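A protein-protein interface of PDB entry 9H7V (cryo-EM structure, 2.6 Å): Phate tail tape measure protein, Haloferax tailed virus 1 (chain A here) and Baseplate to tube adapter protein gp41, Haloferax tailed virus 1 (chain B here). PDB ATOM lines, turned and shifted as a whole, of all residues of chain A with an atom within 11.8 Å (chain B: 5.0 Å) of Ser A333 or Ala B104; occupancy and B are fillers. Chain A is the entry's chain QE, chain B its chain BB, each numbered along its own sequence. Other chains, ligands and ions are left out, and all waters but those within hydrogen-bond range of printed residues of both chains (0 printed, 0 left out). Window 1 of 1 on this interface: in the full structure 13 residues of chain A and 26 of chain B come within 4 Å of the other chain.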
ATOM      1  N   THR A 328     -16.121 -32.886   9.491  1.00  0.00           N
ATOM      2  CA  THR A 328     -15.881 -31.454   9.470  1.00  0.00           C
ATOM      3  C   THR A 328     -17.060 -30.792  10.174  1.00  0.00           C
ATOM      4  O   THR A 328     -18.210 -31.021   9.800  1.00  0.00           O
ATOM      5  CB  THR A 328     -15.746 -30.907   8.039  1.00  0.00           C
ATOM      6  OG1 THR A 328     -17.002 -31.015   7.368  1.00  0.00           O
ATOM      7  CG2 THR A 328     -14.662 -31.581   7.225  1.00  0.00           C
ATOM      8  N   GLY A 329     -16.767 -29.991  11.202  1.00  0.00           N
ATOM      9  CA  GLY A 329     -17.817 -29.389  12.007  1.00  0.00           C
ATOM     10  C   GLY A 329     -18.420 -28.148  11.354  1.00  0.00           C
ATOM     11  O   GLY A 329     -18.742 -27.187  12.051  1.00  0.00           O
ATOM     12  N   ARG A 330     -18.585 -28.185  10.024  1.00  0.00           N
ATOM     13  CA  ARG A 330     -19.017 -27.019   9.272  1.00  0.00           C
ATOM     14  C   ARG A 330     -20.526 -27.042   9.064  1.00  0.00           C
ATOM     15  O   ARG A 330     -21.093 -28.047   8.636  1.00  0.00           O
ATOM     16  CB  ARG A 330     -18.262 -26.890   7.948  1.00  0.00           C
ATOM     17  CG  ARG A 330     -16.951 -26.132   8.077  1.00  0.00           C
ATOM     18  CD  ARG A 330     -16.307 -25.886   6.731  1.00  0.00           C
ATOM     19  NE  ARG A 330     -16.848 -24.722   6.042  1.00  0.00           N
ATOM     20  CZ  ARG A 330     -16.325 -24.183   4.945  1.00  0.00           C
ATOM     21  NH1 ARG A 330     -16.889 -23.123   4.394  1.00  0.00           N
ATOM     22  NH2 ARG A 330     -15.237 -24.701   4.402  1.00  0.00           N
ATOM     23  N   TYR A 331     -21.140 -25.899   9.370  1.00  0.00           N
ATOM     24  CA  TYR A 331     -22.565 -25.698   9.203  1.00  0.00           C
ATOM     25  C   TYR A 331     -22.851 -25.334   7.749  1.00  0.00           C
ATOM     26  O   TYR A 331     -22.010 -24.753   7.063  1.00  0.00           O
ATOM     27  CB  TYR A 331     -23.054 -24.596  10.148  1.00  0.00           C
ATOM     28  CG  TYR A 331     -23.066 -24.908  11.627  1.00  0.00           C
ATOM     29  CD1 TYR A 331     -22.441 -26.030  12.161  1.00  0.00           C
ATOM     30  CD2 TYR A 331     -23.688 -24.039  12.511  1.00  0.00           C
ATOM     31  CE1 TYR A 331     -22.456 -26.289  13.524  1.00  0.00           C
ATOM     32  CE2 TYR A 331     -23.716 -24.285  13.874  1.00  0.00           C
ATOM     33  CZ  TYR A 331     -23.091 -25.409  14.384  1.00  0.00           C
ATOM     34  OH  TYR A 331     -23.109 -25.650  15.725  1.00  0.00           O
ATOM     35  N   ARG A 332     -24.039 -25.741   7.294  1.00  0.00           N
ATOM     36  CA  ARG A 332     -24.708 -25.189   6.127  1.00  0.00           C
ATOM     37  C   ARG A 332     -26.172 -24.954   6.497  1.00  0.00           C
ATOM     38  O   ARG A 332     -26.728 -25.691   7.310  1.00  0.00           O
ATOM     39  CB  ARG A 332     -24.552 -26.106   4.907  1.00  0.00           C
ATOM     40  CG  ARG A 332     -24.991 -27.549   5.120  1.00  0.00           C
ATOM     41  CD  ARG A 332     -25.382 -28.233   3.823  1.00  0.00           C
ATOM     42  NE  ARG A 332     -26.711 -27.840   3.370  1.00  0.00           N
ATOM     43  CZ  ARG A 332     -27.238 -28.119   2.180  1.00  0.00           C
ATOM     44  NH1 ARG A 332     -28.459 -27.705   1.890  1.00  0.00           N
ATOM     45  NH2 ARG A 332     -26.550 -28.801   1.281  1.00  0.00           N
ATOM     46  N   SER A 333     -26.786 -23.923   5.899  1.00  0.00           N
ATOM     47  CA  SER A 333     -28.148 -23.521   6.225  1.00  0.00           C
ATOM     48  C   SER A 333     -28.886 -23.047   4.973  1.00  0.00           C
ATOM     49  O   SER A 333     -28.252 -22.566   4.037  1.00  0.00           O
ATOM     50  CB  SER A 333     -28.153 -22.478   7.314  1.00  0.00           C
ATOM     51  OG  SER A 333     -27.382 -21.345   6.941  1.00  0.00           O
ATOM     52  N   ASP A 334     -30.225 -23.156   4.989  1.00  0.00           N
ATOM     53  CA  ASP A 334     -31.093 -23.061   3.819  1.00  0.00           C
ATOM     54  C   ASP A 334     -30.727 -21.870   2.929  1.00  0.00           C
ATOM     55  O   ASP A 334     -30.572 -20.757   3.430  1.00  0.00           O
ATOM     56  CB  ASP A 334     -32.573 -23.013   4.219  1.00  0.00           C
ATOM     57  CG  ASP A 334     -33.088 -24.240   4.958  1.00  0.00           C
ATOM     58  OD1 ASP A 334     -32.284 -25.160   5.226  1.00  0.00           O
ATOM     59  OD2 ASP A 334     -34.297 -24.269   5.262  1.00  0.00           O
ATOM     60  N   PRO A 335     -30.567 -22.069   1.594  1.00  0.00           N
ATOM     61  CA  PRO A 335     -30.322 -20.969   0.654  1.00  0.00           C
ATOM     62  C   PRO A 335     -31.451 -19.942   0.578  1.00  0.00           C
ATOM     63  O   PRO A 335     -32.600 -20.250   0.894  1.00  0.00           O
ATOM     64  CB  PRO A 335     -30.203 -21.665  -0.712  1.00  0.00           C
ATOM     65  CG  PRO A 335     -29.836 -23.092  -0.379  1.00  0.00           C
ATOM     66  CD  PRO A 335     -30.567 -23.377   0.917  1.00  0.00           C
ATOM     67  N   SER A 336     -31.086 -18.722   0.157  1.00  0.00           N
ATOM     68  CA  SER A 336     -31.987 -17.612  -0.124  1.00  0.00           C
ATOM     69  C   SER A 336     -33.104 -18.070  -1.065  1.00  0.00           C
ATOM     70  O   SER A 336     -32.830 -18.724  -2.071  1.00  0.00           O
ATOM     71  CB  SER A 336     -31.197 -16.467  -0.704  1.00  0.00           C
ATOM     72  OG  SER A 336     -31.992 -15.302  -0.830  1.00  0.00           O
ATOM     73  N   ARG A 337     -34.353 -17.698  -0.738  1.00  0.00           N
ATOM     74  CA  ARG A 337     -35.544 -18.429  -1.158  1.00  0.00           C
ATOM     75  C   ARG A 337     -35.858 -18.272  -2.648  1.00  0.00           C
ATOM     76  O   ARG A 337     -36.112 -19.274  -3.316  1.00  0.00           O
ATOM     77  CB  ARG A 337     -36.754 -18.123  -0.264  1.00  0.00           C
ATOM     78  CG  ARG A 337     -36.643 -18.638   1.167  1.00  0.00           C
ATOM     79  CD  ARG A 337     -36.762 -20.145   1.350  1.00  0.00           C
ATOM     80  NE  ARG A 337     -35.568 -20.859   0.911  1.00  0.00           N
ATOM     81  CZ  ARG A 337     -35.492 -22.162   0.653  1.00  0.00           C
ATOM     82  NH1 ARG A 337     -34.345 -22.685   0.254  1.00  0.00           N
ATOM     83  NH2 ARG A 337     -36.551 -22.942   0.795  1.00  0.00           N
ATOM     84  N   LEU B  55     -27.607 -24.867  15.597  1.00  0.00           N
ATOM     85  CA  LEU B  55     -27.873 -23.961  14.493  1.00  0.00           C
ATOM     86  C   LEU B  55     -29.073 -23.085  14.835  1.00  0.00           C
ATOM     87  O   LEU B  55     -30.059 -23.564  15.393  1.00  0.00           O
ATOM     88  CB  LEU B  55     -28.172 -24.771  13.227  1.00  0.00           C
ATOM     89  CG  LEU B  55     -27.205 -24.600  12.055  1.00  0.00           C
ATOM     90  CD1 LEU B  55     -27.567 -25.541  10.918  1.00  0.00           C
ATOM     91  CD2 LEU B  55     -27.182 -23.161  11.555  1.00  0.00           C
ATOM     92  N   THR B  57     -30.951 -20.358  12.083  1.00  0.00           N
ATOM     93  CA  THR B  57     -30.971 -19.719  10.776  1.00  0.00           C
ATOM     94  C   THR B  57     -32.146 -18.749  10.715  1.00  0.00           C
ATOM     95  O   THR B  57     -33.243 -19.079  11.157  1.00  0.00           O
ATOM     96  CB  THR B  57     -31.090 -20.756   9.650  1.00  0.00           C
ATOM     97  OG1 THR B  57     -30.168 -21.818   9.896  1.00  0.00           O
ATOM     98  CG2 THR B  57     -30.850 -20.182   8.271  1.00  0.00           C
ATOM     99  N   PRO B 102     -23.614 -14.353   6.791  1.00  0.00           N
ATOM    100  CA  PRO B 102     -24.308 -14.863   5.605  1.00  0.00           C
ATOM    101  C   PRO B 102     -24.306 -16.391   5.643  1.00  0.00           C
ATOM    102  O   PRO B 102     -23.344 -16.987   6.127  1.00  0.00           O
ATOM    103  CB  PRO B 102     -23.441 -14.345   4.449  1.00  0.00           C
ATOM    104  CG  PRO B 102     -22.817 -13.082   4.997  1.00  0.00           C
ATOM    105  CD  PRO B 102     -22.549 -13.395   6.454  1.00  0.00           C
ATOM    106  N   ALA B 103     -25.387 -17.005   5.135  1.00  0.00           N
ATOM    107  CA  ALA B 103     -25.674 -18.431   5.261  1.00  0.00           C
ATOM    108  C   ALA B 103     -24.418 -19.275   5.041  1.00  0.00           C
ATOM    109  O   ALA B 103     -23.677 -19.052   4.084  1.00  0.00           O
ATOM    110  CB  ALA B 103     -26.780 -18.820   4.315  1.00  0.00           C
ATOM    111  N   ALA B 104     -24.235 -20.278   5.909  1.00  0.00           N
ATOM    112  CA  ALA B 104     -22.930 -20.784   6.316  1.00  0.00           C
ATOM    113  C   ALA B 104     -22.089 -21.360   5.174  1.00  0.00           C
ATOM    114  O   ALA B 104     -20.872 -21.183   5.177  1.00  0.00           O
ATOM    115  CB  ALA B 104     -23.084 -21.743   7.470  1.00  0.00           C
ATOM    116  N   GLY B 105     -22.720 -22.043   4.210  1.00  0.00           N
ATOM    117  CA  GLY B 105     -21.971 -22.653   3.121  1.00  0.00           C
ATOM    118  C   GLY B 105     -22.543 -22.321   1.747  1.00  0.00           C
ATOM    119  O   GLY B 105     -22.282 -23.034   0.779  1.00  0.00           O
ATOM    120  N   GLN B 106     -23.292 -21.214   1.674  1.00  0.00           N
ATOM    121  CA  GLN B 106     -24.244 -20.992   0.598  1.00  0.00           C
ATOM    122  C   GLN B 106     -23.741 -19.946  -0.392  1.00  0.00           C
ATOM    123  O   GLN B 106     -23.188 -18.919  -0.002  1.00  0.00           O
ATOM    124  CB  GLN B 106     -25.615 -20.631   1.172  1.00  0.00           C
ATOM    125  CG  GLN B 106     -26.564 -21.817   1.292  1.00  0.00           C
ATOM    126  CD  GLN B 106     -26.032 -22.983   2.095  1.00  0.00           C
ATOM    127  OE1 GLN B 106     -25.422 -22.820   3.150  1.00  0.00           O
ATOM    128  NE2 GLN B 106     -26.281 -24.184   1.600  1.00  0.00           N
ATOM    129  N   THR B 129     -27.048 -16.930   9.292  1.00  0.00           N
ATOM    130  CA  THR B 129     -26.738 -17.905  10.330  1.00  0.00           C
ATOM    131  C   THR B 129     -26.342 -17.155  11.600  1.00  0.00           C
ATOM    132  O   THR B 129     -25.540 -16.226  11.539  1.00  0.00           O
ATOM    133  CB  THR B 129     -25.584 -18.819   9.893  1.00  0.00           C
ATOM    134  OG1 THR B 129     -25.895 -19.366   8.611  1.00  0.00           O
ATOM    135  CG2 THR B 129     -25.296 -19.947  10.860  1.00  0.00           C
ATOM    136  N   ARG B 179     -21.190 -15.687   0.596  1.00  0.00           N
ATOM    137  CA  ARG B 179     -19.832 -15.869   1.086  1.00  0.00           C
ATOM    138  C   ARG B 179     -19.629 -17.333   1.479  1.00  0.00           C
ATOM    139  O   ARG B 179     -19.562 -17.646   2.667  1.00  0.00           O
ATOM    140  CB  ARG B 179     -19.565 -14.919   2.258  1.00  0.00           C
ATOM    141  CG  ARG B 179     -19.567 -13.441   1.893  1.00  0.00           C
ATOM    142  CD  ARG B 179     -19.101 -12.545   3.026  1.00  0.00           C
ATOM    143  NE  ARG B 179     -17.853 -13.007   3.618  1.00  0.00           N
ATOM    144  CZ  ARG B 179     -16.632 -12.757   3.152  1.00  0.00           C
ATOM    145  NH1 ARG B 179     -15.584 -13.250   3.785  1.00  0.00           N
ATOM    146  NH2 ARG B 179     -16.456 -12.024   2.066  1.00  0.00           N
ATOM    147  N   PRO B 180     -19.525 -18.282   0.510  1.00  0.00           N
ATOM    148  CA  PRO B 180     -19.412 -19.707   0.836  1.00  0.00           C
ATOM    149  C   PRO B 180     -18.071 -20.160   1.420  1.00  0.00           C
ATOM    150  O   PRO B 180     -17.975 -21.277   1.928  1.00  0.00           O
ATOM    151  CB  PRO B 180     -19.682 -20.404  -0.507  1.00  0.00           C
ATOM    152  CG  PRO B 180     -19.231 -19.404  -1.546  1.00  0.00           C
ATOM    153  CD  PRO B 180     -19.530 -18.048  -0.945  1.00  0.00           C
ATOM    154  N   ASP B 182     -16.416 -18.604   3.882  1.00  0.00           N
ATOM    155  CA  ASP B 182     -16.395 -18.407   5.323  1.00  0.00           C
ATOM    156  C   ASP B 182     -16.760 -19.721   6.005  1.00  0.00           C
ATOM    157  O   ASP B 182     -17.608 -20.462   5.510  1.00  0.00           O
ATOM    158  CB  ASP B 182     -17.376 -17.318   5.765  1.00  0.00           C
ATOM    159  CG  ASP B 182     -16.951 -15.896   5.442  1.00  0.00           C
ATOM    160  OD1 ASP B 182     -15.758 -15.681   5.141  1.00  0.00           O
ATOM    161  OD2 ASP B 182     -17.821 -15.007   5.500  1.00  0.00           O
ATOM    162  N   VAL B 184     -18.330 -21.489   9.341  1.00  0.00           N
ATOM    163  CA  VAL B 184     -19.079 -21.490  10.585  1.00  0.00           C
ATOM    164  C   VAL B 184     -18.857 -22.857  11.229  1.00  0.00           C
ATOM    165  O   VAL B 184     -19.198 -23.881  10.638  1.00  0.00           O
ATOM    166  CB  VAL B 184     -20.568 -21.168  10.336  1.00  0.00           C
ATOM    167  CG1 VAL B 184     -21.422 -21.362  11.573  1.00  0.00           C
ATOM    168  CG2 VAL B 184     -20.760 -19.763   9.785  1.00  0.00           C
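The guanidinium group (NE) of Arg A337 is in hydrogen-bond range of the backbone carbonyl oxygen (O) of Pro A335. The guanidinium group of Arg B179 lies within salt-bridge range of the side-chain carboxylate of Asp B182, 2.7 Å away. OG1 of Thr B129 sits at hydrogen-bond distance from N of Ala B104 (3.3 Å).
Printed residues of chain B that touch a printed residue of chain A: Leu B55, Thr B57, Ala B103, Ala B104, Gly B105, Gln B106, Thr B129, Pro B180, Asp B182 and Val B184. Of the 10 printed residues of chain A, 6 touch a printed residue of chain B. Among the printed residues, no Asp or Glu carboxylate lies within 4 Å of a Lys or Arg side-chain nitrogen of the other chain.
The backbone NH (N) of Ala B104 is in hydrogen-bond range of the side-chain hydroxyl (OG) of Ser A333 (3.5 Å). The backbone NH (N) of Tyr A331 sits at hydrogen-bond distance from the backbone carbonyl oxygen (O) of Val B184. O of Asp B182 sits at hydrogen-bond distance from NH1 of Arg A330. The backbone carbonyl oxygen (O) of Ser A333 sits close to the side-chain amide oxygen (OE1) of Gln B106 (3.0 Å). The guanidinium group (NH1) of Arg A330 is in hydrogen-bond range of the backbone carbonyl oxygen (O) of Pro B180 (3.3 Å). OG1 of Thr B129 is in hydrogen-bond range of OG of Ser A333 (3.0 Å).
O of Gly A329 touches O of Val B184, 3.6 Å away. Arg A330 touches Val B184. Leu B55 touches Tyr A331 (CG to CD2, 3.6 Å). Ala B104 touches Tyr A331. Tyr A331 touches Gly B105 (O to N, 3.998 Å). Arg A332 touches Leu B55. CB of Arg A332 touches OE1 of Gln B106, 3.8 Å away. Ser A333 touches Thr B57 (CB to OG1, 3.3 Å). Ser A333 touches Ala B103 (OG to CB, 3.7 Å). Pro A335 touches Gln B106 (CG to CG, 3.9 Å).
Of chain B, only Thr B57 (3.3 Å), Ala B103 (3.7 Å), Ala B104 (3.5 Å), Gln B106 (3.0 Å) and Thr B129 (3.0 Å) come within 4 Å of Ser A333. Thr B57 touches just one residue of chain A: Ser A333 (3.3 Å). No residue of chain A comes within 4 Å of Pro B102. Gln B106 touches just these residues of chain A: Arg A332 (3.8 Å), Ser A333 (3.0 Å) and Pro A335 (3.9 Å). Of chain A, only Arg A330 comes within 4 Å of Pro B180. Printed residues of chain B within 4 Å of Arg A330: Pro B180, Asp B182 and Val B184. Of the printed residues of chain A, Gly B105 touches Tyr A331. Printed residues of chain A within 4 Å of Leu B55: Tyr A331 and Arg A332. Printed residues of chain B within 4 Å of Pro A335: Gln B106 (3.9 Å). Thr A328 touches none of the printed residues of chain B. The nearest residue of chain A that does not touch Ala B104 is Arg A332 (4.04 Å). The nearest printed residue of chain B that does not touch Gly A329 is Ala B104 (8.3 Å).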
